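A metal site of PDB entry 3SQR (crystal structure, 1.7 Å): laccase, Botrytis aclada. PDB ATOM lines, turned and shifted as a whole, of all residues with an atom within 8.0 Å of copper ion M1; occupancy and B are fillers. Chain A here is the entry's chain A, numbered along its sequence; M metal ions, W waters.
Copper ion M1 is bound by a ring nitrogen (NE2) of His 525, a ring nitrogen (NE2) of His 468, a ring nitrogen (NE2) of His 170 and water W1. Copper ion M1 has four donor atoms within binding distance. Slightly farther from copper ion M1 lies a ring nitrogen (ND1) of His 466 (2.8 Å).
Within 4 Å of copper ion M1: His 170, His 466, His 468 and His 525.
ND1 of His 170 is in hydrogen-bond range of OXT of Ile 580 (3.0 Å). OD2 of Asp 137 is in hydrogen-bond range of ND1 of His 468, at 2.8 Å. The backbone NH of His 468 sits at hydrogen-bond distance from the backbone carbonyl oxygen of Leu 523. O of His 525 is in hydrogen-bond range of N of His 466. ND1 of His 466 sits close to NE2 of His 468 (3.2 Å). A ring nitrogen (NE2) of His 466 sits at hydrogen-bond distance from a ring nitrogen (NE2) of His 126, 3.4 Å away.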
ATOM      1  N   HIS A 124     -14.255 -11.155  -9.879  1.00  0.00           N
ATOM      2  CA  HIS A 124     -15.237 -11.379 -10.907  1.00  0.00           C
ATOM      3  C   HIS A 124     -15.522 -10.044 -11.670  1.00  0.00           C
ATOM      4  O   HIS A 124     -15.567  -8.980 -11.138  1.00  0.00           O
ATOM      5  CB  HIS A 124     -16.519 -11.935 -10.301  1.00  0.00           C
ATOM      6  CG  HIS A 124     -17.669 -11.967 -11.250  1.00  0.00           C
ATOM      7  ND1 HIS A 124     -17.678 -12.788 -12.364  1.00  0.00           N
ATOM      8  CD2 HIS A 124     -18.881 -11.359 -11.217  1.00  0.00           C
ATOM      9  CE1 HIS A 124     -18.810 -12.587 -13.027  1.00  0.00           C
ATOM     10  NE2 HIS A 124     -19.570 -11.756 -12.343  1.00  0.00           N
ATOM     11  N   TRP A 125     -15.722 -10.214 -12.961  1.00  0.00           N
ATOM     12  CA  TRP A 125     -15.931  -9.098 -13.915  1.00  0.00           C
ATOM     13  C   TRP A 125     -17.408  -9.219 -14.248  1.00  0.00           C
ATOM     14  O   TRP A 125     -17.842 -10.110 -14.999  1.00  0.00           O
ATOM     15  CB  TRP A 125     -14.975  -9.274 -15.105  1.00  0.00           C
ATOM     16  CG  TRP A 125     -13.639  -9.755 -14.633  1.00  0.00           C
ATOM     17  CD1 TRP A 125     -13.210 -11.077 -14.534  1.00  0.00           C
ATOM     18  CD2 TRP A 125     -12.602  -8.966 -14.062  1.00  0.00           C
ATOM     19  NE1 TRP A 125     -11.993 -11.106 -13.949  1.00  0.00           N
ATOM     20  CE2 TRP A 125     -11.612  -9.842 -13.604  1.00  0.00           C
ATOM     21  CE3 TRP A 125     -12.452  -7.585 -13.801  1.00  0.00           C
ATOM     22  CZ2 TRP A 125     -10.516  -9.423 -12.930  1.00  0.00           C
ATOM     23  CZ3 TRP A 125     -11.341  -7.151 -13.118  1.00  0.00           C
ATOM     24  CH2 TRP A 125     -10.354  -8.073 -12.701  1.00  0.00           C
ATOM     25  N   HIS A 126     -18.218  -8.380 -13.568  1.00  0.00           N
ATOM     26  CA  HIS A 126     -19.632  -8.617 -13.529  1.00  0.00           C
ATOM     27  C   HIS A 126     -20.276  -8.505 -14.898  1.00  0.00           C
ATOM     28  O   HIS A 126     -20.225  -7.504 -15.566  1.00  0.00           O
ATOM     29  CB  HIS A 126     -20.312  -7.791 -12.428  1.00  0.00           C
ATOM     30  CG  HIS A 126     -21.738  -8.121 -12.298  1.00  0.00           C
ATOM     31  ND1 HIS A 126     -22.302  -8.558 -11.138  1.00  0.00           N
ATOM     32  CD2 HIS A 126     -22.756  -8.000 -13.183  1.00  0.00           C
ATOM     33  CE1 HIS A 126     -23.593  -8.731 -11.319  1.00  0.00           C
ATOM     34  NE2 HIS A 126     -23.896  -8.438 -12.569  1.00  0.00           N
ATOM     35  N   GLY A 127     -21.012  -9.556 -15.246  1.00  0.00           N
ATOM     36  CA  GLY A 127     -21.774  -9.592 -16.460  1.00  0.00           C
ATOM     37  C   GLY A 127     -20.937  -9.872 -17.694  1.00  0.00           C
ATOM     38  O   GLY A 127     -21.481  -9.944 -18.796  1.00  0.00           O
ATOM     39  N   ASP A 137     -13.436 -16.056 -14.933  1.00  0.00           N
ATOM     40  CA  ASP A 137     -14.678 -15.521 -14.392  1.00  0.00           C
ATOM     41  C   ASP A 137     -14.603 -15.049 -12.943  1.00  0.00           C
ATOM     42  O   ASP A 137     -15.404 -14.231 -12.488  1.00  0.00           O
ATOM     43  CB  ASP A 137     -15.807 -16.519 -14.591  1.00  0.00           C
ATOM     44  CG  ASP A 137     -17.149 -15.944 -14.365  1.00  0.00           C
ATOM     45  OD1 ASP A 137     -17.431 -14.809 -14.896  1.00  0.00           O
ATOM     46  OD2 ASP A 137     -17.976 -16.599 -13.701  1.00  0.00           O
ATOM     47  N   GLY A 138     -13.630 -15.574 -12.199  1.00  0.00           N
ATOM     48  CA  GLY A 138     -13.328 -15.125 -10.854  1.00  0.00           C
ATOM     49  C   GLY A 138     -14.248 -15.592  -9.765  1.00  0.00           C
ATOM     50  O   GLY A 138     -14.289 -14.986  -8.715  1.00  0.00           O
ATOM     51  N   VAL A 139     -14.854 -16.802  -9.909  1.00  0.00           N
ATOM     52  CA  VAL A 139     -15.691 -17.316  -8.877  1.00  0.00           C
ATOM     53  C   VAL A 139     -14.868 -18.371  -8.132  1.00  0.00           C
ATOM     54  O   VAL A 139     -14.670 -19.423  -8.717  1.00  0.00           O
ATOM     55  CB  VAL A 139     -16.921 -17.970  -9.350  1.00  0.00           C
ATOM     56  CG1 VAL A 139     -17.808 -18.461  -8.208  1.00  0.00           C
ATOM     57  CG2 VAL A 139     -17.762 -16.881 -10.221  1.00  0.00           C
ATOM     58  N   TRP A 166     -19.126  -3.548 -13.516  1.00  0.00           N
ATOM     59  CA  TRP A 166     -18.282  -3.363 -12.373  1.00  0.00           C
ATOM     60  C   TRP A 166     -17.525  -4.666 -12.196  1.00  0.00           C
ATOM     61  O   TRP A 166     -17.930  -5.666 -12.725  1.00  0.00           O
ATOM     62  CB  TRP A 166     -19.079  -2.992 -11.140  1.00  0.00           C
ATOM     63  CG  TRP A 166     -20.172  -3.945 -10.668  1.00  0.00           C
ATOM     64  CD1 TRP A 166     -21.215  -4.477 -11.410  1.00  0.00           C
ATOM     65  CD2 TRP A 166     -20.390  -4.381  -9.321  1.00  0.00           C
ATOM     66  NE1 TRP A 166     -22.065  -5.184 -10.575  1.00  0.00           N
ATOM     67  CE2 TRP A 166     -21.562  -5.173  -9.315  1.00  0.00           C
ATOM     68  CE3 TRP A 166     -19.704  -4.201  -8.130  1.00  0.00           C
ATOM     69  CZ2 TRP A 166     -22.008  -5.819  -8.142  1.00  0.00           C
ATOM     70  CZ3 TRP A 166     -20.156  -4.789  -6.968  1.00  0.00           C
ATOM     71  CH2 TRP A 166     -21.302  -5.612  -6.970  1.00  0.00           C
ATOM     72  N   HIS A 168     -15.625  -7.047  -9.031  1.00  0.00           N
ATOM     73  CA  HIS A 168     -15.665  -7.098  -7.601  1.00  0.00           C
ATOM     74  C   HIS A 168     -15.166  -8.414  -7.119  1.00  0.00           C
ATOM     75  O   HIS A 168     -15.207  -9.373  -7.833  1.00  0.00           O
ATOM     76  CB  HIS A 168     -17.061  -6.865  -7.046  1.00  0.00           C
ATOM     77  CG  HIS A 168     -18.122  -7.810  -7.548  1.00  0.00           C
ATOM     78  ND1 HIS A 168     -18.377  -9.040  -6.973  1.00  0.00           N
ATOM     79  CD2 HIS A 168     -19.065  -7.648  -8.513  1.00  0.00           C
ATOM     80  CE1 HIS A 168     -19.399  -9.605  -7.607  1.00  0.00           C
ATOM     81  NE2 HIS A 168     -19.858  -8.762  -8.524  1.00  0.00           N
ATOM     82  N   SER A 169     -14.742  -8.444  -5.890  1.00  0.00           N
ATOM     83  CA  SER A 169     -14.414  -9.776  -5.346  1.00  0.00           C
ATOM     84  C   SER A 169     -15.651 -10.643  -5.316  1.00  0.00           C
ATOM     85  O   SER A 169     -16.740 -10.169  -5.001  1.00  0.00           O
ATOM     86  CB  SER A 169     -13.848  -9.673  -3.938  1.00  0.00           C
ATOM     87  OG  SER A 169     -13.724 -10.994  -3.401  1.00  0.00           O
ATOM     88  N   HIS A 170     -15.471 -11.928  -5.659  1.00  0.00           N
ATOM     89  CA  HIS A 170     -16.534 -12.864  -5.526  1.00  0.00           C
ATOM     90  C   HIS A 170     -16.120 -13.884  -4.439  1.00  0.00           C
ATOM     91  O   HIS A 170     -16.707 -14.932  -4.302  1.00  0.00           O
ATOM     92  CB  HIS A 170     -16.795 -13.556  -6.842  1.00  0.00           C
ATOM     93  CG  HIS A 170     -18.228 -13.854  -7.095  1.00  0.00           C
ATOM     94  ND1 HIS A 170     -18.990 -14.607  -6.262  1.00  0.00           N
ATOM     95  CD2 HIS A 170     -19.068 -13.458  -8.106  1.00  0.00           C
ATOM     96  CE1 HIS A 170     -20.205 -14.726  -6.750  1.00  0.00           C
ATOM     97  NE2 HIS A 170     -20.295 -14.013  -7.863  1.00  0.00           N
ATOM     98  N   TYR A 175     -16.644  -7.806  -1.192  1.00  0.00           N
ATOM     99  CA  TYR A 175     -17.037  -6.551  -1.883  1.00  0.00           C
ATOM    100  C   TYR A 175     -17.837  -5.646  -0.970  1.00  0.00           C
ATOM    101  O   TYR A 175     -17.952  -4.416  -1.225  1.00  0.00           O
ATOM    102  CB  TYR A 175     -17.712  -6.779  -3.260  1.00  0.00           C
ATOM    103  CG  TYR A 175     -19.207  -7.047  -3.234  1.00  0.00           C
ATOM    104  CD1 TYR A 175     -20.081  -6.023  -3.133  1.00  0.00           C
ATOM    105  CD2 TYR A 175     -19.710  -8.314  -3.276  1.00  0.00           C
ATOM    106  CE1 TYR A 175     -21.412  -6.198  -3.113  1.00  0.00           C
ATOM    107  CE2 TYR A 175     -21.121  -8.528  -3.246  1.00  0.00           C
ATOM    108  CZ  TYR A 175     -21.943  -7.458  -3.180  1.00  0.00           C
ATOM    109  OH  TYR A 175     -23.326  -7.555  -3.143  1.00  0.00           O
ATOM    110  N   ILE A 465     -31.115 -11.832  -8.821  1.00  0.00           N
ATOM    111  CA  ILE A 465     -30.477 -13.095  -9.207  1.00  0.00           C
ATOM    112  C   ILE A 465     -29.531 -12.754 -10.357  1.00  0.00           C
ATOM    113  O   ILE A 465     -29.952 -12.118 -11.363  1.00  0.00           O
ATOM    114  CB  ILE A 465     -31.528 -14.108  -9.734  1.00  0.00           C
ATOM    115  CG1 ILE A 465     -32.535 -14.417  -8.621  1.00  0.00           C
ATOM    116  CG2 ILE A 465     -30.845 -15.361 -10.331  1.00  0.00           C
ATOM    117  CD1 ILE A 465     -31.890 -15.064  -7.400  1.00  0.00           C
ATOM    118  N   HIS A 466     -28.278 -13.136 -10.192  1.00  0.00           N
ATOM    119  CA  HIS A 466     -27.234 -12.905 -11.159  1.00  0.00           C
ATOM    120  C   HIS A 466     -26.842 -14.245 -11.769  1.00  0.00           C
ATOM    121  O   HIS A 466     -26.561 -15.197 -11.025  1.00  0.00           O
ATOM    122  CB  HIS A 466     -26.021 -12.318 -10.445  1.00  0.00           C
ATOM    123  CG  HIS A 466     -24.823 -12.170 -11.332  1.00  0.00           C
ATOM    124  ND1 HIS A 466     -23.521 -12.301 -10.881  1.00  0.00           N
ATOM    125  CD2 HIS A 466     -24.759 -11.817 -12.630  1.00  0.00           C
ATOM    126  CE1 HIS A 466     -22.711 -12.121 -11.915  1.00  0.00           C
ATOM    127  NE2 HIS A 466     -23.443 -11.820 -12.975  1.00  0.00           N
ATOM    128  N   LEU A 467     -26.806 -14.280 -13.088  1.00  0.00           N
ATOM    129  CA  LEU A 467     -26.302 -15.446 -13.832  1.00  0.00           C
ATOM    130  C   LEU A 467     -24.958 -15.109 -14.467  1.00  0.00           C
ATOM    131  O   LEU A 467     -24.840 -14.134 -15.149  1.00  0.00           O
ATOM    132  CB  LEU A 467     -27.264 -15.797 -14.975  1.00  0.00           C
ATOM    133  CG  LEU A 467     -26.779 -16.939 -15.934  1.00  0.00           C
ATOM    134  CD1 LEU A 467     -26.529 -18.236 -15.223  1.00  0.00           C
ATOM    135  CD2 LEU A 467     -27.808 -17.246 -17.037  1.00  0.00           C
ATOM    136  N   HIS A 468     -23.948 -15.945 -14.254  1.00  0.00           N
ATOM    137  CA  HIS A 468     -22.641 -15.762 -14.843  1.00  0.00           C
ATOM    138  C   HIS A 468     -22.628 -16.383 -16.267  1.00  0.00           C
ATOM    139  O   HIS A 468     -23.405 -17.293 -16.576  1.00  0.00           O
ATOM    140  CB  HIS A 468     -21.611 -16.463 -13.953  1.00  0.00           C
ATOM    141  CG  HIS A 468     -21.330 -15.763 -12.681  1.00  0.00           C
ATOM    142  ND1 HIS A 468     -20.059 -15.417 -12.287  1.00  0.00           N
ATOM    143  CD2 HIS A 468     -22.157 -15.344 -11.697  1.00  0.00           C
ATOM    144  CE1 HIS A 468     -20.125 -14.769 -11.140  1.00  0.00           C
ATOM    145  NE2 HIS A 468     -21.371 -14.725 -10.759  1.00  0.00           N
ATOM    146  N   ASP A 500     -28.255  -9.342 -17.072  1.00  0.00           N
ATOM    147  CA  ASP A 500     -27.599 -10.398 -16.252  1.00  0.00           C
ATOM    148  C   ASP A 500     -27.908 -10.461 -14.769  1.00  0.00           C
ATOM    149  O   ASP A 500     -27.562 -11.432 -14.104  1.00  0.00           O
ATOM    150  CB  ASP A 500     -26.060 -10.337 -16.482  1.00  0.00           C
ATOM    151  CG  ASP A 500     -25.437  -9.022 -16.058  1.00  0.00           C
ATOM    152  OD1 ASP A 500     -25.497  -8.748 -14.844  1.00  0.00           O
ATOM    153  OD2 ASP A 500     -24.918  -8.285 -16.959  1.00  0.00           O
ATOM    154  N   VAL A 501     -28.679  -9.478 -14.282  1.00  0.00           N
ATOM    155  CA  VAL A 501     -29.203  -9.529 -12.891  1.00  0.00           C
ATOM    156  C   VAL A 501     -30.687  -9.190 -12.946  1.00  0.00           C
ATOM    157  O   VAL A 501     -31.092  -8.186 -13.537  1.00  0.00           O
ATOM    158  CB  VAL A 501     -28.497  -8.573 -11.916  1.00  0.00           C
ATOM    159  CG1 VAL A 501     -29.164  -8.622 -10.574  1.00  0.00           C
ATOM    160  CG2 VAL A 501     -27.044  -8.886 -11.761  1.00  0.00           C
ATOM    161  N   LEU A 523     -22.026 -19.849 -12.247  1.00  0.00           N
ATOM    162  CA  LEU A 523     -22.712 -19.594 -11.001  1.00  0.00           C
ATOM    163  C   LEU A 523     -23.997 -18.790 -11.241  1.00  0.00           C
ATOM    164  O   LEU A 523     -24.045 -17.900 -12.110  1.00  0.00           O
ATOM    165  CB  LEU A 523     -21.805 -18.833 -10.042  1.00  0.00           C
ATOM    166  CG  LEU A 523     -22.339 -18.637  -8.624  1.00  0.00           C
ATOM    167  CD1 LEU A 523     -22.428 -20.042  -7.916  1.00  0.00           C
ATOM    168  CD2 LEU A 523     -21.460 -17.692  -7.843  1.00  0.00           C
ATOM    169  N   LEU A 524     -25.059 -19.124 -10.512  1.00  0.00           N
ATOM    170  CA  LEU A 524     -26.247 -18.283 -10.480  1.00  0.00           C
ATOM    171  C   LEU A 524     -26.578 -18.126  -8.999  1.00  0.00           C
ATOM    172  O   LEU A 524     -26.552 -19.082  -8.259  1.00  0.00           O
ATOM    173  CB  LEU A 524     -27.417 -18.949 -11.206  1.00  0.00           C
ATOM    174  CG  LEU A 524     -28.759 -18.217 -11.029  1.00  0.00           C
ATOM    175  CD1 LEU A 524     -29.581 -18.310 -12.310  1.00  0.00           C
ATOM    176  CD2 LEU A 524     -29.500 -18.768  -9.769  1.00  0.00           C
ATOM    177  N   HIS A 525     -26.811 -16.902  -8.565  1.00  0.00           N
ATOM    178  CA  HIS A 525     -26.979 -16.662  -7.179  1.00  0.00           C
ATOM    179  C   HIS A 525     -27.691 -15.371  -6.920  1.00  0.00           C
ATOM    180  O   HIS A 525     -27.734 -14.502  -7.784  1.00  0.00           O
ATOM    181  CB  HIS A 525     -25.635 -16.616  -6.483  1.00  0.00           C
ATOM    182  CG  HIS A 525     -24.774 -15.483  -6.914  1.00  0.00           C
ATOM    183  ND1 HIS A 525     -24.597 -14.345  -6.162  1.00  0.00           N
ATOM    184  CD2 HIS A 525     -24.052 -15.302  -8.045  1.00  0.00           C
ATOM    185  CE1 HIS A 525     -23.754 -13.543  -6.786  1.00  0.00           C
ATOM    186  NE2 HIS A 525     -23.442 -14.085  -7.952  1.00  0.00           N
ATOM    187  N   CYS A 526     -28.292 -15.299  -5.730  1.00  0.00           N
ATOM    188  CA  CYS A 526     -28.757 -14.015  -5.212  1.00  0.00           C
ATOM    189  C   CYS A 526     -27.531 -13.138  -4.920  1.00  0.00           C
ATOM    190  O   CYS A 526     -26.531 -13.618  -4.343  1.00  0.00           O
ATOM    191  CB  CYS A 526     -29.545 -14.224  -3.916  1.00  0.00           C
ATOM    192  SG  CYS A 526     -30.098 -12.667  -3.312  1.00  0.00           S
ATOM    193  N   HIS A 527     -27.600 -11.889  -5.338  1.00  0.00           N
ATOM    194  CA  HIS A 527     -26.503 -10.953  -5.197  1.00  0.00           C
ATOM    195  C   HIS A 527     -26.570 -10.182  -3.881  1.00  0.00           C
ATOM    196  O   HIS A 527     -25.688  -9.318  -3.609  1.00  0.00           O
ATOM    197  CB  HIS A 527     -26.475  -9.935  -6.386  1.00  0.00           C
ATOM    198  CG  HIS A 527     -25.091  -9.598  -6.864  1.00  0.00           C
ATOM    199  ND1 HIS A 527     -24.167  -9.011  -6.045  1.00  0.00           N
ATOM    200  CD2 HIS A 527     -24.486  -9.736  -8.092  1.00  0.00           C
ATOM    201  CE1 HIS A 527     -23.050  -8.813  -6.723  1.00  0.00           C
ATOM    202  NE2 HIS A 527     -23.203  -9.262  -7.965  1.00  0.00           N
ATOM    203  N   ALA A 532     -26.038 -14.831  -0.708  1.00  0.00           N
ATOM    204  CA  ALA A 532     -24.997 -15.598  -1.383  1.00  0.00           C
ATOM    205  C   ALA A 532     -24.170 -16.386  -0.409  1.00  0.00           C
ATOM    206  O   ALA A 532     -23.920 -17.581  -0.592  1.00  0.00           O
ATOM    207  CB  ALA A 532     -24.081 -14.633  -2.259  1.00  0.00           C
ATOM    208  N   ILE A 580     -18.910 -18.310  -1.971  1.00  0.00           N
ATOM    209  CA  ILE A 580     -19.082 -17.415  -3.126  1.00  0.00           C
ATOM    210  C   ILE A 580     -19.411 -16.051  -2.648  1.00  0.00           C
ATOM    211  O   ILE A 580     -19.368 -15.802  -1.403  1.00  0.00           O
ATOM    212  CB  ILE A 580     -20.240 -17.863  -4.092  1.00  0.00           C
ATOM    213  CG1 ILE A 580     -21.594 -17.961  -3.366  1.00  0.00           C
ATOM    214  CG2 ILE A 580     -19.856 -19.100  -4.910  1.00  0.00           C
ATOM    215  CD1 ILE A 580     -22.783 -17.725  -4.271  1.00  0.00           C
ATOM    216  OXT ILE A 580     -19.820 -15.206  -3.471  1.00  0.00           O
HETATM  217 CU    CU M   1     -21.886 -13.690  -9.132  1.00  0.00          CU
HETATM  218 CU    CU M   2     -21.645  -9.100  -9.352  1.00  0.00          CU
HETATM  219  O   HOH W   1     -21.566 -11.665  -8.730  1.00  0.00           O
